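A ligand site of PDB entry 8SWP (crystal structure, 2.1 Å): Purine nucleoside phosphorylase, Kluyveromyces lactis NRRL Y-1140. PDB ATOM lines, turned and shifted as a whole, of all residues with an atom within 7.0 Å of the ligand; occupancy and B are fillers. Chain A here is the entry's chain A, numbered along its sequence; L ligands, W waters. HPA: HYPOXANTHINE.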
ATOM      1  N   SER A  43      -3.579 -24.286  -9.597  1.00  0.00           N
ATOM      2  CA  SER A  43      -2.723 -25.099 -10.462  1.00  0.00           C
ATOM      3  C   SER A  43      -1.381 -25.350  -9.791  1.00  0.00           C
ATOM      4  O   SER A  43      -0.768 -24.430  -9.225  1.00  0.00           O
ATOM      5  CB  SER A  43      -2.519 -24.400 -11.801  1.00  0.00           C
ATOM      6  OG  SER A  43      -3.755 -23.939 -12.323  1.00  0.00           O
ATOM      7  N   ASN A 129      -1.886 -20.346  -9.345  1.00  0.00           N
ATOM      8  CA  ASN A 129      -2.792 -20.401 -10.485  1.00  0.00           C
ATOM      9  C   ASN A 129      -1.973 -20.647 -11.738  1.00  0.00           C
ATOM     10  O   ASN A 129      -0.748 -20.524 -11.740  1.00  0.00           O
ATOM     11  CB  ASN A 129      -3.624 -19.122 -10.618  1.00  0.00           C
ATOM     12  CG  ASN A 129      -2.784 -17.863 -10.582  1.00  0.00           C
ATOM     13  OD1 ASN A 129      -2.659 -17.213  -9.551  1.00  0.00           O
ATOM     14  ND2 ASN A 129      -2.183 -17.529 -11.720  1.00  0.00           N
ATOM     15  N   ALA A 130      -2.672 -21.002 -12.818  1.00  0.00           N
ATOM     16  CA  ALA A 130      -2.073 -21.062 -14.134  1.00  0.00           C
ATOM     17  C   ALA A 130      -2.169 -19.710 -14.811  1.00  0.00           C
ATOM     18  O   ALA A 130      -3.059 -18.905 -14.501  1.00  0.00           O
ATOM     19  CB  ALA A 130      -2.764 -22.132 -14.988  1.00  0.00           C
ATOM     20  N   ALA A 131      -1.252 -19.448 -15.725  1.00  0.00           N
ATOM     21  CA  ALA A 131      -1.220 -18.165 -16.414  1.00  0.00           C
ATOM     22  C   ALA A 131      -0.565 -18.315 -17.774  1.00  0.00           C
ATOM     23  O   ALA A 131       0.343 -19.133 -17.956  1.00  0.00           O
ATOM     24  CB  ALA A 131      -0.487 -17.097 -15.581  1.00  0.00           C
ATOM     25  N   GLY A 132      -1.030 -17.516 -18.729  1.00  0.00           N
ATOM     26  CA  GLY A 132      -0.412 -17.440 -20.036  1.00  0.00           C
ATOM     27  C   GLY A 132       0.677 -16.385 -20.028  1.00  0.00           C
ATOM     28  O   GLY A 132       0.474 -15.281 -19.530  1.00  0.00           O
ATOM     29  N   GLY A 133       1.830 -16.732 -20.585  1.00  0.00           N
ATOM     30  CA  GLY A 133       2.953 -15.819 -20.615  1.00  0.00           C
ATOM     31  C   GLY A 133       2.790 -14.694 -21.623  1.00  0.00           C
ATOM     32  O   GLY A 133       2.734 -14.937 -22.824  1.00  0.00           O
ATOM     33  N   ILE A 134       2.703 -13.469 -21.126  1.00  0.00           N
ATOM     34  CA  ILE A 134       2.637 -12.286 -21.973  1.00  0.00           C
ATOM     35  C   ILE A 134       4.020 -11.667 -22.180  1.00  0.00           C
ATOM     36  O   ILE A 134       4.345 -11.213 -23.271  1.00  0.00           O
ATOM     37  CB  ILE A 134       1.642 -11.266 -21.399  1.00  0.00           C
ATOM     38  CG1 ILE A 134       0.220 -11.804 -21.470  1.00  0.00           C
ATOM     39  CG2 ILE A 134       1.737  -9.936 -22.136  1.00  0.00           C
ATOM     40  CD1 ILE A 134      -0.371 -11.783 -22.873  1.00  0.00           C
ATOM     41  N   TYR A 206       0.873  -9.692 -12.837  1.00  0.00           N
ATOM     42  CA  TYR A 206      -0.164 -10.633 -13.200  1.00  0.00           C
ATOM     43  C   TYR A 206      -1.450  -9.873 -13.511  1.00  0.00           C
ATOM     44  O   TYR A 206      -1.867  -9.014 -12.736  1.00  0.00           O
ATOM     45  CB  TYR A 206      -0.406 -11.635 -12.073  1.00  0.00           C
ATOM     46  CG  TYR A 206      -1.603 -12.540 -12.238  1.00  0.00           C
ATOM     47  CD1 TYR A 206      -1.515 -13.713 -12.997  1.00  0.00           C
ATOM     48  CD2 TYR A 206      -2.811 -12.248 -11.632  1.00  0.00           C
ATOM     49  CE1 TYR A 206      -2.607 -14.550 -13.145  1.00  0.00           C
ATOM     50  CE2 TYR A 206      -3.911 -13.078 -11.780  1.00  0.00           C
ATOM     51  CZ  TYR A 206      -3.804 -14.217 -12.528  1.00  0.00           C
ATOM     52  OH  TYR A 206      -4.893 -15.049 -12.663  1.00  0.00           O
ATOM     53  N   SER A 207      -2.076 -10.172 -14.647  1.00  0.00           N
ATOM     54  CA  SER A 207      -3.308  -9.523 -15.050  1.00  0.00           C
ATOM     55  C   SER A 207      -4.470 -10.513 -14.950  1.00  0.00           C
ATOM     56  O   SER A 207      -4.388 -11.617 -15.488  1.00  0.00           O
ATOM     57  CB  SER A 207      -3.217  -8.947 -16.461  1.00  0.00           C
ATOM     58  OG  SER A 207      -2.450  -7.754 -16.477  1.00  0.00           O
ATOM     59  N   VAL A 209      -8.106 -11.576 -15.962  1.00  0.00           N
ATOM     60  CA  VAL A 209      -9.188 -11.425 -16.931  1.00  0.00           C
ATOM     61  C   VAL A 209     -10.279 -12.436 -16.566  1.00  0.00           C
ATOM     62  O   VAL A 209     -10.028 -13.437 -15.879  1.00  0.00           O
ATOM     63  CB  VAL A 209      -8.721 -11.634 -18.381  1.00  0.00           C
ATOM     64  CG1 VAL A 209      -7.633 -10.625 -18.737  1.00  0.00           C
ATOM     65  CG2 VAL A 209      -8.235 -13.057 -18.604  1.00  0.00           C
ATOM     66  N   GLY A 211     -12.320 -14.454 -18.470  1.00  0.00           N
ATOM     67  CA  GLY A 211     -12.445 -15.714 -19.163  1.00  0.00           C
ATOM     68  C   GLY A 211     -13.870 -15.925 -19.636  1.00  0.00           C
ATOM     69  O   GLY A 211     -14.692 -15.001 -19.623  1.00  0.00           O
ATOM     70  N   THR A 213     -12.651 -17.531 -22.264  1.00  0.00           N
ATOM     71  CA  THR A 213     -11.926 -17.600 -23.528  1.00  0.00           C
ATOM     72  C   THR A 213     -10.451 -17.285 -23.317  1.00  0.00           C
ATOM     73  O   THR A 213     -10.087 -16.471 -22.456  1.00  0.00           O
ATOM     74  CB  THR A 213     -12.506 -16.623 -24.554  1.00  0.00           C
ATOM     75  OG1 THR A 213     -12.741 -15.354 -23.940  1.00  0.00           O
ATOM     76  CG2 THR A 213     -13.799 -17.168 -25.128  1.00  0.00           C
ATOM     77  N   PHE A 214      -9.604 -17.941 -24.092  1.00  0.00           N
ATOM     78  CA  PHE A 214      -8.212 -17.521 -24.186  1.00  0.00           C
ATOM     79  C   PHE A 214      -8.141 -16.236 -25.001  1.00  0.00           C
ATOM     80  O   PHE A 214      -8.974 -15.975 -25.866  1.00  0.00           O
ATOM     81  CB  PHE A 214      -7.356 -18.619 -24.811  1.00  0.00           C
ATOM     82  CG  PHE A 214      -7.176 -19.822 -23.928  1.00  0.00           C
ATOM     83  CD1 PHE A 214      -6.454 -19.740 -22.755  1.00  0.00           C
ATOM     84  CD2 PHE A 214      -7.738 -21.034 -24.283  1.00  0.00           C
ATOM     85  CE1 PHE A 214      -6.293 -20.853 -21.945  1.00  0.00           C
ATOM     86  CE2 PHE A 214      -7.580 -22.153 -23.484  1.00  0.00           C
ATOM     87  CZ  PHE A 214      -6.852 -22.064 -22.309  1.00  0.00           C
ATOM     88  N   GLU A 215      -7.119 -15.432 -24.720  1.00  0.00           N
ATOM     89  CA  GLU A 215      -7.038 -14.105 -25.315  1.00  0.00           C
ATOM     90  C   GLU A 215      -6.795 -14.190 -26.809  1.00  0.00           C
ATOM     91  O   GLU A 215      -6.050 -15.045 -27.291  1.00  0.00           O
ATOM     92  CB  GLU A 215      -5.922 -13.274 -24.659  1.00  0.00           C
ATOM     93  CG  GLU A 215      -6.111 -12.961 -23.182  1.00  0.00           C
ATOM     94  CD  GLU A 215      -6.028 -14.196 -22.319  1.00  0.00           C
ATOM     95  OE1 GLU A 215      -5.263 -15.106 -22.681  1.00  0.00           O
ATOM     96  OE2 GLU A 215      -6.741 -14.264 -21.297  1.00  0.00           O
ATOM     97  N   SER A 220      -4.101 -10.033 -26.253  1.00  0.00           N
ATOM     98  CA  SER A 220      -2.788 -10.264 -25.669  1.00  0.00           C
ATOM     99  C   SER A 220      -1.855  -9.091 -25.940  1.00  0.00           C
ATOM    100  O   SER A 220      -1.059  -8.708 -25.070  1.00  0.00           O
ATOM    101  CB  SER A 220      -2.193 -11.556 -26.206  1.00  0.00           C
ATOM    102  OG  SER A 220      -2.836 -12.691 -25.645  1.00  0.00           O
ATOM    103  N   VAL A 231      -1.028 -13.462 -17.774  1.00  0.00           N
ATOM    104  CA  VAL A 231      -2.473 -13.246 -17.723  1.00  0.00           C
ATOM    105  C   VAL A 231      -3.140 -14.528 -17.237  1.00  0.00           C
ATOM    106  O   VAL A 231      -2.813 -15.631 -17.703  1.00  0.00           O
ATOM    107  CB  VAL A 231      -3.032 -12.826 -19.097  1.00  0.00           C
ATOM    108  CG1 VAL A 231      -2.635 -13.819 -20.185  1.00  0.00           C
ATOM    109  CG2 VAL A 231      -4.539 -12.659 -19.030  1.00  0.00           C
ATOM    110  N   GLY A 232      -4.063 -14.388 -16.282  1.00  0.00           N
ATOM    111  CA  GLY A 232      -4.767 -15.513 -15.714  1.00  0.00           C
ATOM    112  C   GLY A 232      -6.229 -15.196 -15.460  1.00  0.00           C
ATOM    113  O   GLY A 232      -6.682 -14.064 -15.671  1.00  0.00           O
ATOM    114  N   MET A 233      -6.948 -16.200 -14.978  1.00  0.00           N
ATOM    115  CA  MET A 233      -8.394 -16.138 -14.862  1.00  0.00           C
ATOM    116  C   MET A 233      -8.899 -16.159 -13.422  1.00  0.00           C
ATOM    117  O   MET A 233     -10.088 -16.384 -13.188  1.00  0.00           O
ATOM    118  CB  MET A 233      -9.006 -17.308 -15.651  1.00  0.00           C
ATOM    119  CG  MET A 233      -9.341 -17.008 -17.095  1.00  0.00           C
ATOM    120  SD  MET A 233     -10.105 -18.577 -17.986  1.00  0.00           S
ATOM    121  CE  MET A 233      -9.226 -18.407 -19.723  1.00  0.00           C
ATOM    122  N   SER A 234      -8.010 -15.946 -12.455  1.00  0.00           N
ATOM    123  CA  SER A 234      -8.373 -16.097 -11.055  1.00  0.00           C
ATOM    124  C   SER A 234      -7.450 -15.248 -10.184  1.00  0.00           C
ATOM    125  O   SER A 234      -6.766 -14.338 -10.671  1.00  0.00           O
ATOM    126  CB  SER A 234      -8.324 -17.579 -10.645  1.00  0.00           C
ATOM    127  OG  SER A 234      -6.986 -18.026 -10.556  1.00  0.00           O
ATOM    128  N   LEU A 254       1.958 -20.187 -12.491  1.00  0.00           N
ATOM    129  CA  LEU A 254       2.612 -21.207 -13.299  1.00  0.00           C
ATOM    130  C   LEU A 254       2.413 -20.854 -14.762  1.00  0.00           C
ATOM    131  O   LEU A 254       1.286 -20.856 -15.267  1.00  0.00           O
ATOM    132  CB  LEU A 254       2.038 -22.596 -12.997  1.00  0.00           C
ATOM    133  CG  LEU A 254       2.469 -23.362 -11.740  1.00  0.00           C
ATOM    134  CD1 LEU A 254       2.005 -22.671 -10.463  1.00  0.00           C
ATOM    135  CD2 LEU A 254       1.954 -24.790 -11.787  1.00  0.00           C
ATOM    136  N   ILE A 255       3.505 -20.520 -15.450  1.00  0.00           N
ATOM    137  CA  ILE A 255       3.436 -20.216 -16.879  1.00  0.00           C
ATOM    138  C   ILE A 255       3.174 -21.509 -17.634  1.00  0.00           C
ATOM    139  O   ILE A 255       4.080 -22.317 -17.836  1.00  0.00           O
ATOM    140  CB  ILE A 255       4.721 -19.518 -17.368  1.00  0.00           C
ATOM    141  CG1 ILE A 255       5.101 -18.363 -16.441  1.00  0.00           C
ATOM    142  CG2 ILE A 255       4.535 -19.018 -18.801  1.00  0.00           C
ATOM    143  CD1 ILE A 255       4.048 -17.269 -16.360  1.00  0.00           C
ATOM    144  N   THR A 256       1.929 -21.702 -18.068  1.00  0.00           N
ATOM    145  CA  THR A 256       1.505 -22.937 -18.707  1.00  0.00           C
ATOM    146  C   THR A 256       1.528 -22.864 -20.228  1.00  0.00           C
ATOM    147  O   THR A 256       1.412 -23.908 -20.879  1.00  0.00           O
ATOM    148  CB  THR A 256       0.099 -23.328 -18.244  1.00  0.00           C
ATOM    149  OG1 THR A 256      -0.802 -22.245 -18.472  1.00  0.00           O
ATOM    150  CG2 THR A 256       0.118 -23.666 -16.761  1.00  0.00           C
ATOM    151  N   ASN A 257       1.656 -21.674 -20.804  1.00  0.00           N
ATOM    152  CA  ASN A 257       1.652 -21.507 -22.252  1.00  0.00           C
ATOM    153  C   ASN A 257       2.132 -20.103 -22.585  1.00  0.00           C
ATOM    154  O   ASN A 257       2.099 -19.199 -21.746  1.00  0.00           O
ATOM    155  CB  ASN A 257       0.249 -21.733 -22.838  1.00  0.00           C
ATOM    156  CG  ASN A 257      -0.797 -20.821 -22.233  1.00  0.00           C
ATOM    157  OD1 ASN A 257      -1.092 -20.917 -21.047  1.00  0.00           O
ATOM    158  ND2 ASN A 257      -1.337 -19.915 -23.042  1.00  0.00           N
ATOM    159  N   GLU A 258       2.592 -19.939 -23.822  1.00  0.00           N
ATOM    160  CA  GLU A 258       3.045 -18.651 -24.329  1.00  0.00           C
ATOM    161  C   GLU A 258       1.941 -18.065 -25.203  1.00  0.00           C
ATOM    162  O   GLU A 258       1.529 -18.679 -26.196  1.00  0.00           O
ATOM    163  CB  GLU A 258       4.349 -18.799 -25.116  1.00  0.00           C
ATOM    164  CG  GLU A 258       5.528 -19.235 -24.258  1.00  0.00           C
ATOM    165  CD  GLU A 258       6.568 -19.994 -25.045  1.00  0.00           C
ATOM    166  OE1 GLU A 258       7.117 -19.425 -26.017  1.00  0.00           O
ATOM    167  OE2 GLU A 258       6.855 -21.159 -24.695  1.00  0.00           O
ATOM    168  N   CYS A 259       1.470 -16.875 -24.831  1.00  0.00           N
ATOM    169  CA  CYS A 259       0.338 -16.273 -25.510  1.00  0.00           C
ATOM    170  C   CYS A 259       0.693 -15.902 -26.945  1.00  0.00           C
ATOM    171  O   CYS A 259       1.789 -15.401 -27.225  1.00  0.00           O
ATOM    172  CB  CYS A 259      -0.130 -15.034 -24.751  1.00  0.00           C
ATOM    173  SG  CYS A 259      -0.808 -15.378 -23.111  1.00  0.00           S
ATOM    174  N   VAL A 260      -0.244 -16.147 -27.867  1.00  0.00           N
ATOM    175  CA  VAL A 260      -0.073 -15.777 -29.264  1.00  0.00           C
ATOM    176  C   VAL A 260      -0.310 -14.281 -29.395  1.00  0.00           C
ATOM    177  O   VAL A 260      -1.433 -13.804 -29.215  1.00  0.00           O
ATOM    178  CB  VAL A 260      -1.016 -16.577 -30.174  1.00  0.00           C
ATOM    179  CG1 VAL A 260      -0.741 -16.235 -31.634  1.00  0.00           C
ATOM    180  CG2 VAL A 260      -0.861 -18.062 -29.926  1.00  0.00           C
ATOM    181  N   ALA A 280      -3.774 -21.693 -27.780  1.00  0.00           N
ATOM    182  CA  ALA A 280      -3.855 -22.189 -26.414  1.00  0.00           C
ATOM    183  C   ALA A 280      -4.908 -23.297 -26.308  1.00  0.00           C
ATOM    184  O   ALA A 280      -5.917 -23.295 -27.014  1.00  0.00           O
ATOM    185  CB  ALA A 280      -4.192 -21.056 -25.452  1.00  0.00           C
ATOM    186  N   THR A 281      -4.650 -24.246 -25.422  1.00  0.00           N
ATOM    187  CA  THR A 281      -5.614 -25.308 -25.180  1.00  0.00           C
ATOM    188  C   THR A 281      -5.598 -25.679 -23.714  1.00  0.00           C
ATOM    189  O   THR A 281      -4.580 -25.514 -23.017  1.00  0.00           O
ATOM    190  CB  THR A 281      -5.352 -26.543 -26.074  1.00  0.00           C
ATOM    191  OG1 THR A 281      -6.560 -27.284 -26.233  1.00  0.00           O
ATOM    192  CG2 THR A 281      -4.294 -27.444 -25.469  1.00  0.00           C
ATOM    193  N   VAL A 285      -2.597 -26.496 -20.684  1.00  0.00           N
ATOM    194  CA  VAL A 285      -2.580 -25.849 -19.376  1.00  0.00           C
ATOM    195  C   VAL A 285      -2.547 -26.899 -18.262  1.00  0.00           C
ATOM    196  O   VAL A 285      -1.752 -26.802 -17.319  1.00  0.00           O
ATOM    197  CB  VAL A 285      -3.796 -24.920 -19.220  1.00  0.00           C
ATOM    198  CG1 VAL A 285      -3.894 -24.399 -17.797  1.00  0.00           C
ATOM    199  CG2 VAL A 285      -3.708 -23.763 -20.211  1.00  0.00           C
ATOM    200  N   SER A 289       0.734 -27.601 -15.820  1.00  0.00           N
ATOM    201  CA  SER A 289       0.536 -27.430 -14.393  1.00  0.00           C
ATOM    202  C   SER A 289       0.945 -28.695 -13.631  1.00  0.00           C
ATOM    203  O   SER A 289       1.525 -28.607 -12.535  1.00  0.00           O
ATOM    204  CB  SER A 289      -0.931 -27.085 -14.093  1.00  0.00           C
ATOM    205  OG  SER A 289      -1.297 -25.866 -14.706  1.00  0.00           O
HETATM  206  N1  HPA L   1      -4.917 -16.901 -20.681  1.00  0.00           N
HETATM  207  C2  HPA L   1      -5.686 -16.777 -19.585  1.00  0.00           C
HETATM  208  N3  HPA L   1      -5.645 -17.594 -18.572  1.00  0.00           N
HETATM  209  C4  HPA L   1      -4.766 -18.609 -18.662  1.00  0.00           C
HETATM  210  C5  HPA L   1      -3.928 -18.808 -19.764  1.00  0.00           C
HETATM  211  C6  HPA L   1      -3.983 -17.911 -20.871  1.00  0.00           C
HETATM  212  O6  HPA L   1      -3.310 -17.958 -21.903  1.00  0.00           O
HETATM  213  N7  HPA L   1      -3.196 -19.932 -19.471  1.00  0.00           N
HETATM  214  C8  HPA L   1      -3.595 -20.353 -18.266  1.00  0.00           C
HETATM  215  N9  HPA L   1      -4.542 -19.604 -17.729  1.00  0.00           N
HETATM  216  O   HOH W   1      -5.838 -18.975 -15.417  1.00  0.00           O
HETATM  217  O   HOH W   2      -3.979 -17.069 -24.634  1.00  0.00           O
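N1 of the ligand sits at hydrogen-bond distance from OE1 of Glu 215, 2.7 Å away. The side-chain amide oxygen (OD1) of Asn 257 lies within hydrogen-bond range of a nitrogen (N7) of the ligand. The backbone NH (N) of Gly 132 sits close to a nitrogen (N7) of the ligand (3.3 Å). A nitrogen (N7) of the ligand sits close to the side-chain hydroxyl (OG1) of Thr 256, at 3.5 Å. SG of Cys 259 lies within hydrogen-bond range of O6 of the ligand.
The backbone carbonyl oxygen (O) of Asn 257 lies within hydrogen-bond range of the backbone NH (N) of Gly 133, at 2.7 Å. The backbone NH (N) of Gly 132 lies within hydrogen-bond range of the backbone carbonyl oxygen (O) of Val 231 (2.8 Å). N of Thr 256 is in hydrogen-bond range of O of Ala 131 (3.0 Å). N of Ala 130 sits at hydrogen-bond distance from OG of Ser 43, at 3.2 Å. The backbone carbonyl oxygen (O) of Gly 232 lies within hydrogen-bond range of the backbone NH (N) of Val 209, 2.9 Å away. The backbone NH (N) of Gly 232 lies within hydrogen-bond range of the backbone carbonyl oxygen (O) of Ser 207 (2.9 Å). O of Gly 133 is in hydrogen-bond range of N of Cys 259 (3.1 Å). The backbone carbonyl oxygen of Val 285 sits at hydrogen-bond distance from the side-chain hydroxyl of Ser 289 (2.8 Å).
Ala 130 touches the ligand. Ala 131 touches the ligand (C to N7, 3.5 Å). Phe 214 touches the ligand (CD1 to C6, 3.6 Å). Val 231 touches the ligand. CA of Gly 232 touches N3 of the ligand, 3.6 Å away. CE of Met 233 touches N3 of the ligand, at 3.8 Å. CG2 of Val 285 touches C8 of the ligand, 3.9 Å away. Hydrophobic or aromatic side chains that line the ligand: Ala 130, Phe 214, Val 231, Met 233 and Val 285. 12 residues have an atom within 4 Å of the ligand: Ala 130, Ala 131, Gly 132, Phe 214, Glu 215, Val 231, Gly 232, Met 233, Thr 256, Asn 257, Cys 259 and Val 285. The nearest printed residue that does not touch the ligand is Val 209 (4.6 Å).
Water W1 lies within hydrogen-bond range of a nitrogen (N9) of the ligand (2.7 Å), the backbone carbonyl oxygen of Ala 130 (2.9 Å) and the backbone NH of Met 233 (3.0 Å). Water W2 bridges O6 of the ligand (2.9 Å) and OE1 of Glu 215 (3.1 Å).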
